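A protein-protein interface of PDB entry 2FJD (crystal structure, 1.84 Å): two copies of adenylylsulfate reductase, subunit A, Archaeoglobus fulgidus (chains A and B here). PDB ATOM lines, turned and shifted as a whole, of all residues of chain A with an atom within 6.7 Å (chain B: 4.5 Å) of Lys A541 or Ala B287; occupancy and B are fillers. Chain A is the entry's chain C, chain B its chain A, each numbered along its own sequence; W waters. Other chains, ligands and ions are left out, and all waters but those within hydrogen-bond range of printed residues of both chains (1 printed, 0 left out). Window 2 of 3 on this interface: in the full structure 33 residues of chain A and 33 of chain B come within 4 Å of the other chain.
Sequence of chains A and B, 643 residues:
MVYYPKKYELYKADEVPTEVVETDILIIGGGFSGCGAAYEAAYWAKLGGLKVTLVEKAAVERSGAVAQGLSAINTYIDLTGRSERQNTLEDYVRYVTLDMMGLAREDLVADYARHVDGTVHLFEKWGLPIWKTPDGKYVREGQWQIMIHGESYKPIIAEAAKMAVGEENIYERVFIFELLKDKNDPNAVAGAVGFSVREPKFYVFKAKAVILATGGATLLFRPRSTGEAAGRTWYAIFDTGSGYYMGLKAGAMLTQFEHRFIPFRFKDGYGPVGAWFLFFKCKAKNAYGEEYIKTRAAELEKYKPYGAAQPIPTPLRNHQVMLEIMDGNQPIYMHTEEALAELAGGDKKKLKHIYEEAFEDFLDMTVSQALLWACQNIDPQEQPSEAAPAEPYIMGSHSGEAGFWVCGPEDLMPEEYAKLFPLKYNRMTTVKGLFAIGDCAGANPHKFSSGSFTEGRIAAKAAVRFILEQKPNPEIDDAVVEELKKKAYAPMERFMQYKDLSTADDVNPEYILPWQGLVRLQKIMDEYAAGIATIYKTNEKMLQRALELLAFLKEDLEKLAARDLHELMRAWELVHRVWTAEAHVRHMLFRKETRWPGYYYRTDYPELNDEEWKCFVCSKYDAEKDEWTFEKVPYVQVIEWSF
The backbone carbonyl oxygen of Gln B330 sits at hydrogen-bond distance from the side-chain amide nitrogen of Asn A539 (2.9 Å).
NH2 of Arg A602 is in salt-bridge range of OD2 of Asp A604 (2.8 Å). N of Tyr B288 sits at hydrogen-bond distance from OD1 of Asn B286 (2.9 Å). N of Ala B287 sits at hydrogen-bond distance from O of Asn B329 (2.9 Å). The backbone NH (N) of Ala B287 sits at hydrogen-bond distance from the backbone carbonyl oxygen (O) of Pro B331. The backbone NH of Glu A540 is in hydrogen-bond range of the side-chain carboxylate of Asp A604 (3.0 Å). OE1 of Gln A544 sits close to NZ of Lys A541 (3.0 Å).
No position is printed for both chains.
Among the printed residues, merely in contact across the chains: Met A542 with Gln B330 (3.4 Å), Lys A541 with Ala B287 (3.7 Å), Asp A604 with Tyr B288 (3.7 Å), Asn A539 with Tyr B288 (3.8 Å) and Lys A541 with Pro B331 (3.8 Å).
Water W1 lies within hydrogen-bond range of OH of Tyr B288, N of Lys A541, OD1 of Asn A539 and N of Glu A540.
Of the 13 printed residues of chain A, 4 touch a printed residue of chain B. Printed residues of chain A that touch a printed residue of chain B: Asn A539, Lys A541, Met A542 and Asp A604. Hydrophobic or aromatic side chains of chain A within 4 Å of the printed part of chain B: Met A542. Of the 8 printed residues of chain B, 4 touch a printed residue of chain A. Printed residues of chain B that touch a printed residue of chain A: Ala B287, Tyr B288, Gln B330 and Pro B331. Hydrophobic or aromatic side chains of chain B within 4 Å of the printed part of chain A: Ala B287, Tyr B288 and Pro B331. Among the printed residues, 6 pairs touch across the chains. Among the printed residues, no Asp or Glu carboxylate lies within 4 Å of a Lys or Arg side-chain nitrogen of the other chain.
Printed residues of chain B within 4 Å of Asn A539: Tyr B288 and Gln B330. Lys A541 touches just these residues of chain B: Ala B287 (3.7 Å) and Pro B331 (3.8 Å). Printed residues of chain B within 4 Å of Met A542: Gln B330 (3.4 Å). Leu A543 touches none of the printed residues of chain B. Printed residues of chain B within 4 Å of Asp A604: Tyr B288. Ala B287 touches one residue of chain A. Of the printed residues of chain A, Tyr B288 touches Asn A539 and Asp A604. Asn B329 touches none of the printed residues of chain A. Of the printed residues of chain A, Gln B330 touches Asn A539 and Met A542. The nearest residue of chain A that does not touch Ala B287 is Asn A539 (4.9 Å). The nearest printed residue of chain A that does not touch Gln B330 is Lys A541 (4.3 Å).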
ATOM      1  N   TYR A 528     -31.821 -19.577 -25.058  1.00  0.00           N
ATOM      2  CA  TYR A 528     -30.532 -20.231 -25.275  1.00  0.00           C
ATOM      3  C   TYR A 528     -30.448 -21.260 -26.398  1.00  0.00           C
ATOM      4  O   TYR A 528     -29.351 -21.570 -26.868  1.00  0.00           O
ATOM      5  CB  TYR A 528     -30.062 -20.901 -23.980  1.00  0.00           C
ATOM      6  CG  TYR A 528     -29.918 -19.946 -22.820  1.00  0.00           C
ATOM      7  CD1 TYR A 528     -30.978 -19.715 -21.941  1.00  0.00           C
ATOM      8  CD2 TYR A 528     -28.726 -19.263 -22.609  1.00  0.00           C
ATOM      9  CE1 TYR A 528     -30.850 -18.825 -20.878  1.00  0.00           C
ATOM     10  CE2 TYR A 528     -28.585 -18.369 -21.554  1.00  0.00           C
ATOM     11  CZ  TYR A 528     -29.651 -18.157 -20.692  1.00  0.00           C
ATOM     12  OH  TYR A 528     -29.510 -17.273 -19.651  1.00  0.00           O
ATOM     13  N   THR A 538     -27.624 -19.346 -31.965  1.00  0.00           N
ATOM     14  CA  THR A 538     -27.141 -19.871 -30.697  1.00  0.00           C
ATOM     15  C   THR A 538     -25.672 -20.202 -30.888  1.00  0.00           C
ATOM     16  O   THR A 538     -25.139 -20.055 -31.991  1.00  0.00           O
ATOM     17  CB  THR A 538     -27.932 -21.135 -30.246  1.00  0.00           C
ATOM     18  OG1 THR A 538     -27.520 -21.515 -28.928  1.00  0.00           O
ATOM     19  CG2 THR A 538     -27.702 -22.292 -31.196  1.00  0.00           C
ATOM     20  N   ASN A 539     -25.011 -20.606 -29.809  1.00  0.00           N
ATOM     21  CA  ASN A 539     -23.603 -20.977 -29.871  1.00  0.00           C
ATOM     22  C   ASN A 539     -23.320 -21.963 -28.751  1.00  0.00           C
ATOM     23  O   ASN A 539     -24.211 -22.279 -27.966  1.00  0.00           O
ATOM     24  CB  ASN A 539     -22.694 -19.745 -29.741  1.00  0.00           C
ATOM     25  CG  ASN A 539     -22.904 -18.986 -28.440  1.00  0.00           C
ATOM     26  OD1 ASN A 539     -23.021 -19.582 -27.372  1.00  0.00           O
ATOM     27  ND2 ASN A 539     -22.934 -17.656 -28.527  1.00  0.00           N
ATOM     28  N   GLU A 540     -22.082 -22.443 -28.674  1.00  0.00           N
ATOM     29  CA  GLU A 540     -21.707 -23.406 -27.644  1.00  0.00           C
ATOM     30  C   GLU A 540     -22.014 -22.940 -26.221  1.00  0.00           C
ATOM     31  O   GLU A 540     -22.580 -23.695 -25.430  1.00  0.00           O
ATOM     32  CB  GLU A 540     -20.218 -23.745 -27.745  1.00  0.00           C
ATOM     33  CG  GLU A 540     -19.766 -24.769 -26.711  1.00  0.00           C
ATOM     34  CD  GLU A 540     -18.265 -24.973 -26.708  1.00  0.00           C
ATOM     35  OE1 GLU A 540     -17.536 -24.008 -26.397  1.00  0.00           O
ATOM     36  OE2 GLU A 540     -17.819 -26.094 -27.018  1.00  0.00           O
ATOM     37  N   LYS A 541     -21.625 -21.709 -25.893  1.00  0.00           N
ATOM     38  CA  LYS A 541     -21.848 -21.161 -24.560  1.00  0.00           C
ATOM     39  C   LYS A 541     -23.328 -21.111 -24.200  1.00  0.00           C
ATOM     40  O   LYS A 541     -23.719 -21.505 -23.095  1.00  0.00           O
ATOM     41  CB  LYS A 541     -21.245 -19.754 -24.464  1.00  0.00           C
ATOM     42  CG  LYS A 541     -19.751 -19.674 -24.779  1.00  0.00           C
ATOM     43  CD  LYS A 541     -18.881 -20.095 -23.598  1.00  0.00           C
ATOM     44  CE  LYS A 541     -19.039 -21.566 -23.254  1.00  0.00           C
ATOM     45  NZ  LYS A 541     -18.250 -21.949 -22.046  1.00  0.00           N
ATOM     46  N   MET A 542     -24.158 -20.626 -25.121  1.00  0.00           N
ATOM     47  CA  MET A 542     -25.597 -20.549 -24.868  1.00  0.00           C
ATOM     48  C   MET A 542     -26.207 -21.936 -24.673  1.00  0.00           C
ATOM     49  O   MET A 542     -26.999 -22.159 -23.752  1.00  0.00           O
ATOM     50  CB  MET A 542     -26.299 -19.829 -26.027  1.00  0.00           C
ATOM     51  CG  MET A 542     -26.045 -18.330 -26.070  1.00  0.00           C
ATOM     52  SD  MET A 542     -26.625 -17.574 -27.603  1.00  0.00           S
ATOM     53  CE  MET A 542     -28.410 -17.936 -27.523  1.00  0.00           C
ATOM     54  N   LEU A 543     -25.833 -22.876 -25.532  1.00  0.00           N
ATOM     55  CA  LEU A 543     -26.352 -24.235 -25.422  1.00  0.00           C
ATOM     56  C   LEU A 543     -25.901 -24.897 -24.121  1.00  0.00           C
ATOM     57  O   LEU A 543     -26.662 -25.634 -23.500  1.00  0.00           O
ATOM     58  CB  LEU A 543     -25.904 -25.070 -26.622  1.00  0.00           C
ATOM     59  CG  LEU A 543     -26.466 -24.598 -27.965  1.00  0.00           C
ATOM     60  CD1 LEU A 543     -25.738 -25.298 -29.103  1.00  0.00           C
ATOM     61  CD2 LEU A 543     -27.970 -24.884 -28.021  1.00  0.00           C
ATOM     62  N   GLN A 544     -24.665 -24.635 -23.706  1.00  0.00           N
ATOM     63  CA  GLN A 544     -24.161 -25.208 -22.461  1.00  0.00           C
ATOM     64  C   GLN A 544     -24.945 -24.641 -21.283  1.00  0.00           C
ATOM     65  O   GLN A 544     -25.234 -25.355 -20.321  1.00  0.00           O
ATOM     66  CB  GLN A 544     -22.666 -24.916 -22.290  1.00  0.00           C
ATOM     67  CG  GLN A 544     -21.788 -25.634 -23.306  1.00  0.00           C
ATOM     68  CD  GLN A 544     -20.307 -25.419 -23.069  1.00  0.00           C
ATOM     69  OE1 GLN A 544     -19.847 -24.288 -22.922  1.00  0.00           O
ATOM     70  NE2 GLN A 544     -19.549 -26.509 -23.042  1.00  0.00           N
ATOM     71  N   ARG A 545     -25.297 -23.361 -21.357  1.00  0.00           N
ATOM     72  CA  ARG A 545     -26.064 -22.751 -20.277  1.00  0.00           C
ATOM     73  C   ARG A 545     -27.469 -23.338 -20.277  1.00  0.00           C
ATOM     74  O   ARG A 545     -28.068 -23.537 -19.222  1.00  0.00           O
ATOM     75  CB  ARG A 545     -26.119 -21.229 -20.437  1.00  0.00           C
ATOM     76  CG  ARG A 545     -26.890 -20.515 -19.325  1.00  0.00           C
ATOM     77  CD  ARG A 545     -26.417 -20.938 -17.928  1.00  0.00           C
ATOM     78  NE  ARG A 545     -27.057 -20.157 -16.868  1.00  0.00           N
ATOM     79  CZ  ARG A 545     -26.985 -20.448 -15.571  1.00  0.00           C
ATOM     80  NH1 ARG A 545     -26.303 -21.509 -15.161  1.00  0.00           N
ATOM     81  NH2 ARG A 545     -27.586 -19.670 -14.679  1.00  0.00           N
ATOM     82  N   ALA A 546     -27.996 -23.616 -21.466  1.00  0.00           N
ATOM     83  CA  ALA A 546     -29.325 -24.207 -21.570  1.00  0.00           C
ATOM     84  C   ALA A 546     -29.335 -25.534 -20.810  1.00  0.00           C
ATOM     85  O   ALA A 546     -30.281 -25.831 -20.083  1.00  0.00           O
ATOM     86  CB  ALA A 546     -29.695 -24.435 -23.040  1.00  0.00           C
ATOM     87  N   LEU A 589     -25.673 -28.940 -29.938  1.00  0.00           N
ATOM     88  CA  LEU A 589     -24.340 -28.705 -29.398  1.00  0.00           C
ATOM     89  C   LEU A 589     -23.296 -29.604 -30.065  1.00  0.00           C
ATOM     90  O   LEU A 589     -22.169 -29.174 -30.337  1.00  0.00           O
ATOM     91  CB  LEU A 589     -24.349 -28.945 -27.886  1.00  0.00           C
ATOM     92  CG  LEU A 589     -23.035 -28.758 -27.122  1.00  0.00           C
ATOM     93  CD1 LEU A 589     -22.509 -27.346 -27.335  1.00  0.00           C
ATOM     94  CD2 LEU A 589     -23.268 -29.024 -25.640  1.00  0.00           C
ATOM     95  N   ARG A 602     -25.601 -21.478 -35.864  1.00  0.00           N
ATOM     96  CA  ARG A 602     -24.620 -21.595 -34.800  1.00  0.00           C
ATOM     97  C   ARG A 602     -23.635 -20.496 -35.179  1.00  0.00           C
ATOM     98  O   ARG A 602     -22.876 -20.627 -36.144  1.00  0.00           O
ATOM     99  CB  ARG A 602     -23.947 -22.968 -34.783  1.00  0.00           C
ATOM    100  CG  ARG A 602     -24.766 -23.993 -34.016  1.00  0.00           C
ATOM    101  CD  ARG A 602     -23.928 -25.132 -33.484  1.00  0.00           C
ATOM    102  NE  ARG A 602     -22.895 -24.686 -32.548  1.00  0.00           N
ATOM    103  CZ  ARG A 602     -22.178 -25.516 -31.796  1.00  0.00           C
ATOM    104  NH1 ARG A 602     -22.391 -26.825 -31.870  1.00  0.00           N
ATOM    105  NH2 ARG A 602     -21.234 -25.050 -30.990  1.00  0.00           N
ATOM    106  N   ASP A 604     -21.017 -19.674 -33.884  1.00  0.00           N
ATOM    107  CA  ASP A 604     -19.621 -20.076 -33.707  1.00  0.00           C
ATOM    108  C   ASP A 604     -19.137 -21.037 -34.799  1.00  0.00           C
ATOM    109  O   ASP A 604     -17.937 -21.279 -34.939  1.00  0.00           O
ATOM    110  CB  ASP A 604     -19.393 -20.660 -32.299  1.00  0.00           C
ATOM    111  CG  ASP A 604     -20.405 -21.734 -31.914  1.00  0.00           C
ATOM    112  OD1 ASP A 604     -21.482 -21.835 -32.542  1.00  0.00           O
ATOM    113  OD2 ASP A 604     -20.118 -22.471 -30.945  1.00  0.00           O
ATOM    114  N   LYS B 285     -18.077  -8.748 -20.099  1.00  0.00           N
ATOM    115  CA  LYS B 285     -17.424  -9.402 -21.231  1.00  0.00           C
ATOM    116  C   LYS B 285     -18.411 -10.320 -21.936  1.00  0.00           C
ATOM    117  O   LYS B 285     -19.356 -10.805 -21.315  1.00  0.00           O
ATOM    118  CB  LYS B 285     -16.228 -10.226 -20.748  1.00  0.00           C
ATOM    119  CG  LYS B 285     -15.190  -9.425 -19.980  1.00  0.00           C
ATOM    120  CD  LYS B 285     -14.074 -10.329 -19.469  1.00  0.00           C
ATOM    121  CE  LYS B 285     -13.021  -9.532 -18.718  1.00  0.00           C
ATOM    122  NZ  LYS B 285     -11.901 -10.408 -18.260  1.00  0.00           N
ATOM    123  N   ASN B 286     -18.225 -10.533 -23.232  1.00  0.00           N
ATOM    124  CA  ASN B 286     -19.133 -11.416 -23.942  1.00  0.00           C
ATOM    125  C   ASN B 286     -18.774 -12.857 -23.611  1.00  0.00           C
ATOM    126  O   ASN B 286     -17.878 -13.116 -22.803  1.00  0.00           O
ATOM    127  CB  ASN B 286     -19.083 -11.178 -25.457  1.00  0.00           C
ATOM    128  CG  ASN B 286     -17.705 -11.379 -26.042  1.00  0.00           C
ATOM    129  OD1 ASN B 286     -16.859 -12.061 -25.462  1.00  0.00           O
ATOM    130  ND2 ASN B 286     -17.478 -10.799 -27.218  1.00  0.00           N
ATOM    131  N   ALA B 287     -19.470 -13.792 -24.242  1.00  0.00           N
ATOM    132  CA  ALA B 287     -19.256 -15.212 -23.992  1.00  0.00           C
ATOM    133  C   ALA B 287     -17.824 -15.686 -24.206  1.00  0.00           C
ATOM    134  O   ALA B 287     -17.423 -16.711 -23.657  1.00  0.00           O
ATOM    135  CB  ALA B 287     -20.202 -16.032 -24.862  1.00  0.00           C
ATOM    136  N   TYR B 288     -17.053 -14.940 -24.991  1.00  0.00           N
ATOM    137  CA  TYR B 288     -15.679 -15.330 -25.278  1.00  0.00           C
ATOM    138  C   TYR B 288     -14.625 -14.601 -24.460  1.00  0.00           C
ATOM    139  O   TYR B 288     -13.430 -14.729 -24.723  1.00  0.00           O
ATOM    140  CB  TYR B 288     -15.401 -15.159 -26.772  1.00  0.00           C
ATOM    141  CG  TYR B 288     -16.419 -15.885 -27.617  1.00  0.00           C
ATOM    142  CD1 TYR B 288     -17.458 -15.193 -28.242  1.00  0.00           C
ATOM    143  CD2 TYR B 288     -16.386 -17.275 -27.734  1.00  0.00           C
ATOM    144  CE1 TYR B 288     -18.444 -15.871 -28.962  1.00  0.00           C
ATOM    145  CE2 TYR B 288     -17.368 -17.962 -28.449  1.00  0.00           C
ATOM    146  CZ  TYR B 288     -18.393 -17.254 -29.057  1.00  0.00           C
ATOM    147  OH  TYR B 288     -19.372 -17.929 -29.749  1.00  0.00           O
ATOM    148  N   GLY B 289     -15.072 -13.834 -23.470  1.00  0.00           N
ATOM    149  CA  GLY B 289     -14.141 -13.122 -22.614  1.00  0.00           C
ATOM    150  C   GLY B 289     -13.686 -11.762 -23.103  1.00  0.00           C
ATOM    151  O   GLY B 289     -12.759 -11.183 -22.536  1.00  0.00           O
ATOM    152  N   ASN B 329     -22.871 -13.132 -29.585  1.00  0.00           N
ATOM    153  CA  ASN B 329     -21.802 -13.331 -28.617  1.00  0.00           C
ATOM    154  C   ASN B 329     -22.284 -13.442 -27.174  1.00  0.00           C
ATOM    155  O   ASN B 329     -21.527 -13.195 -26.236  1.00  0.00           O
ATOM    156  CB  ASN B 329     -20.757 -12.219 -28.744  1.00  0.00           C
ATOM    157  CG  ASN B 329     -20.041 -12.251 -30.084  1.00  0.00           C
ATOM    158  OD1 ASN B 329     -20.024 -13.277 -30.761  1.00  0.00           O
ATOM    159  ND2 ASN B 329     -19.434 -11.132 -30.464  1.00  0.00           N
ATOM    160  N   GLN B 330     -23.548 -13.813 -26.998  1.00  0.00           N
ATOM    161  CA  GLN B 330     -24.089 -13.991 -25.658  1.00  0.00           C
ATOM    162  C   GLN B 330     -23.672 -15.378 -25.169  1.00  0.00           C
ATOM    163  O   GLN B 330     -23.333 -16.248 -25.970  1.00  0.00           O
ATOM    164  CB  GLN B 330     -25.617 -13.864 -25.668  1.00  0.00           C
ATOM    165  CG  GLN B 330     -26.101 -12.426 -25.801  1.00  0.00           C
ATOM    166  CD  GLN B 330     -27.609 -12.293 -25.680  1.00  0.00           C
ATOM    167  OE1 GLN B 330     -28.360 -12.738 -26.552  1.00  0.00           O
ATOM    168  NE2 GLN B 330     -28.062 -11.684 -24.589  1.00  0.00           N
ATOM    169  N   PRO B 331     -23.708 -15.607 -23.847  1.00  0.00           N
ATOM    170  CA  PRO B 331     -24.116 -14.653 -22.811  1.00  0.00           C
ATOM    171  C   PRO B 331     -23.116 -13.535 -22.554  1.00  0.00           C
ATOM    172  O   PRO B 331     -21.916 -13.680 -22.794  1.00  0.00           O
ATOM    173  CB  PRO B 331     -24.270 -15.531 -21.563  1.00  0.00           C
ATOM    174  CG  PRO B 331     -24.394 -16.937 -22.104  1.00  0.00           C
ATOM    175  CD  PRO B 331     -23.441 -16.928 -23.258  1.00  0.00           C
HETATM  176  O   HOH W   1     -19.810 -20.096 -27.860  1.00  0.00           O
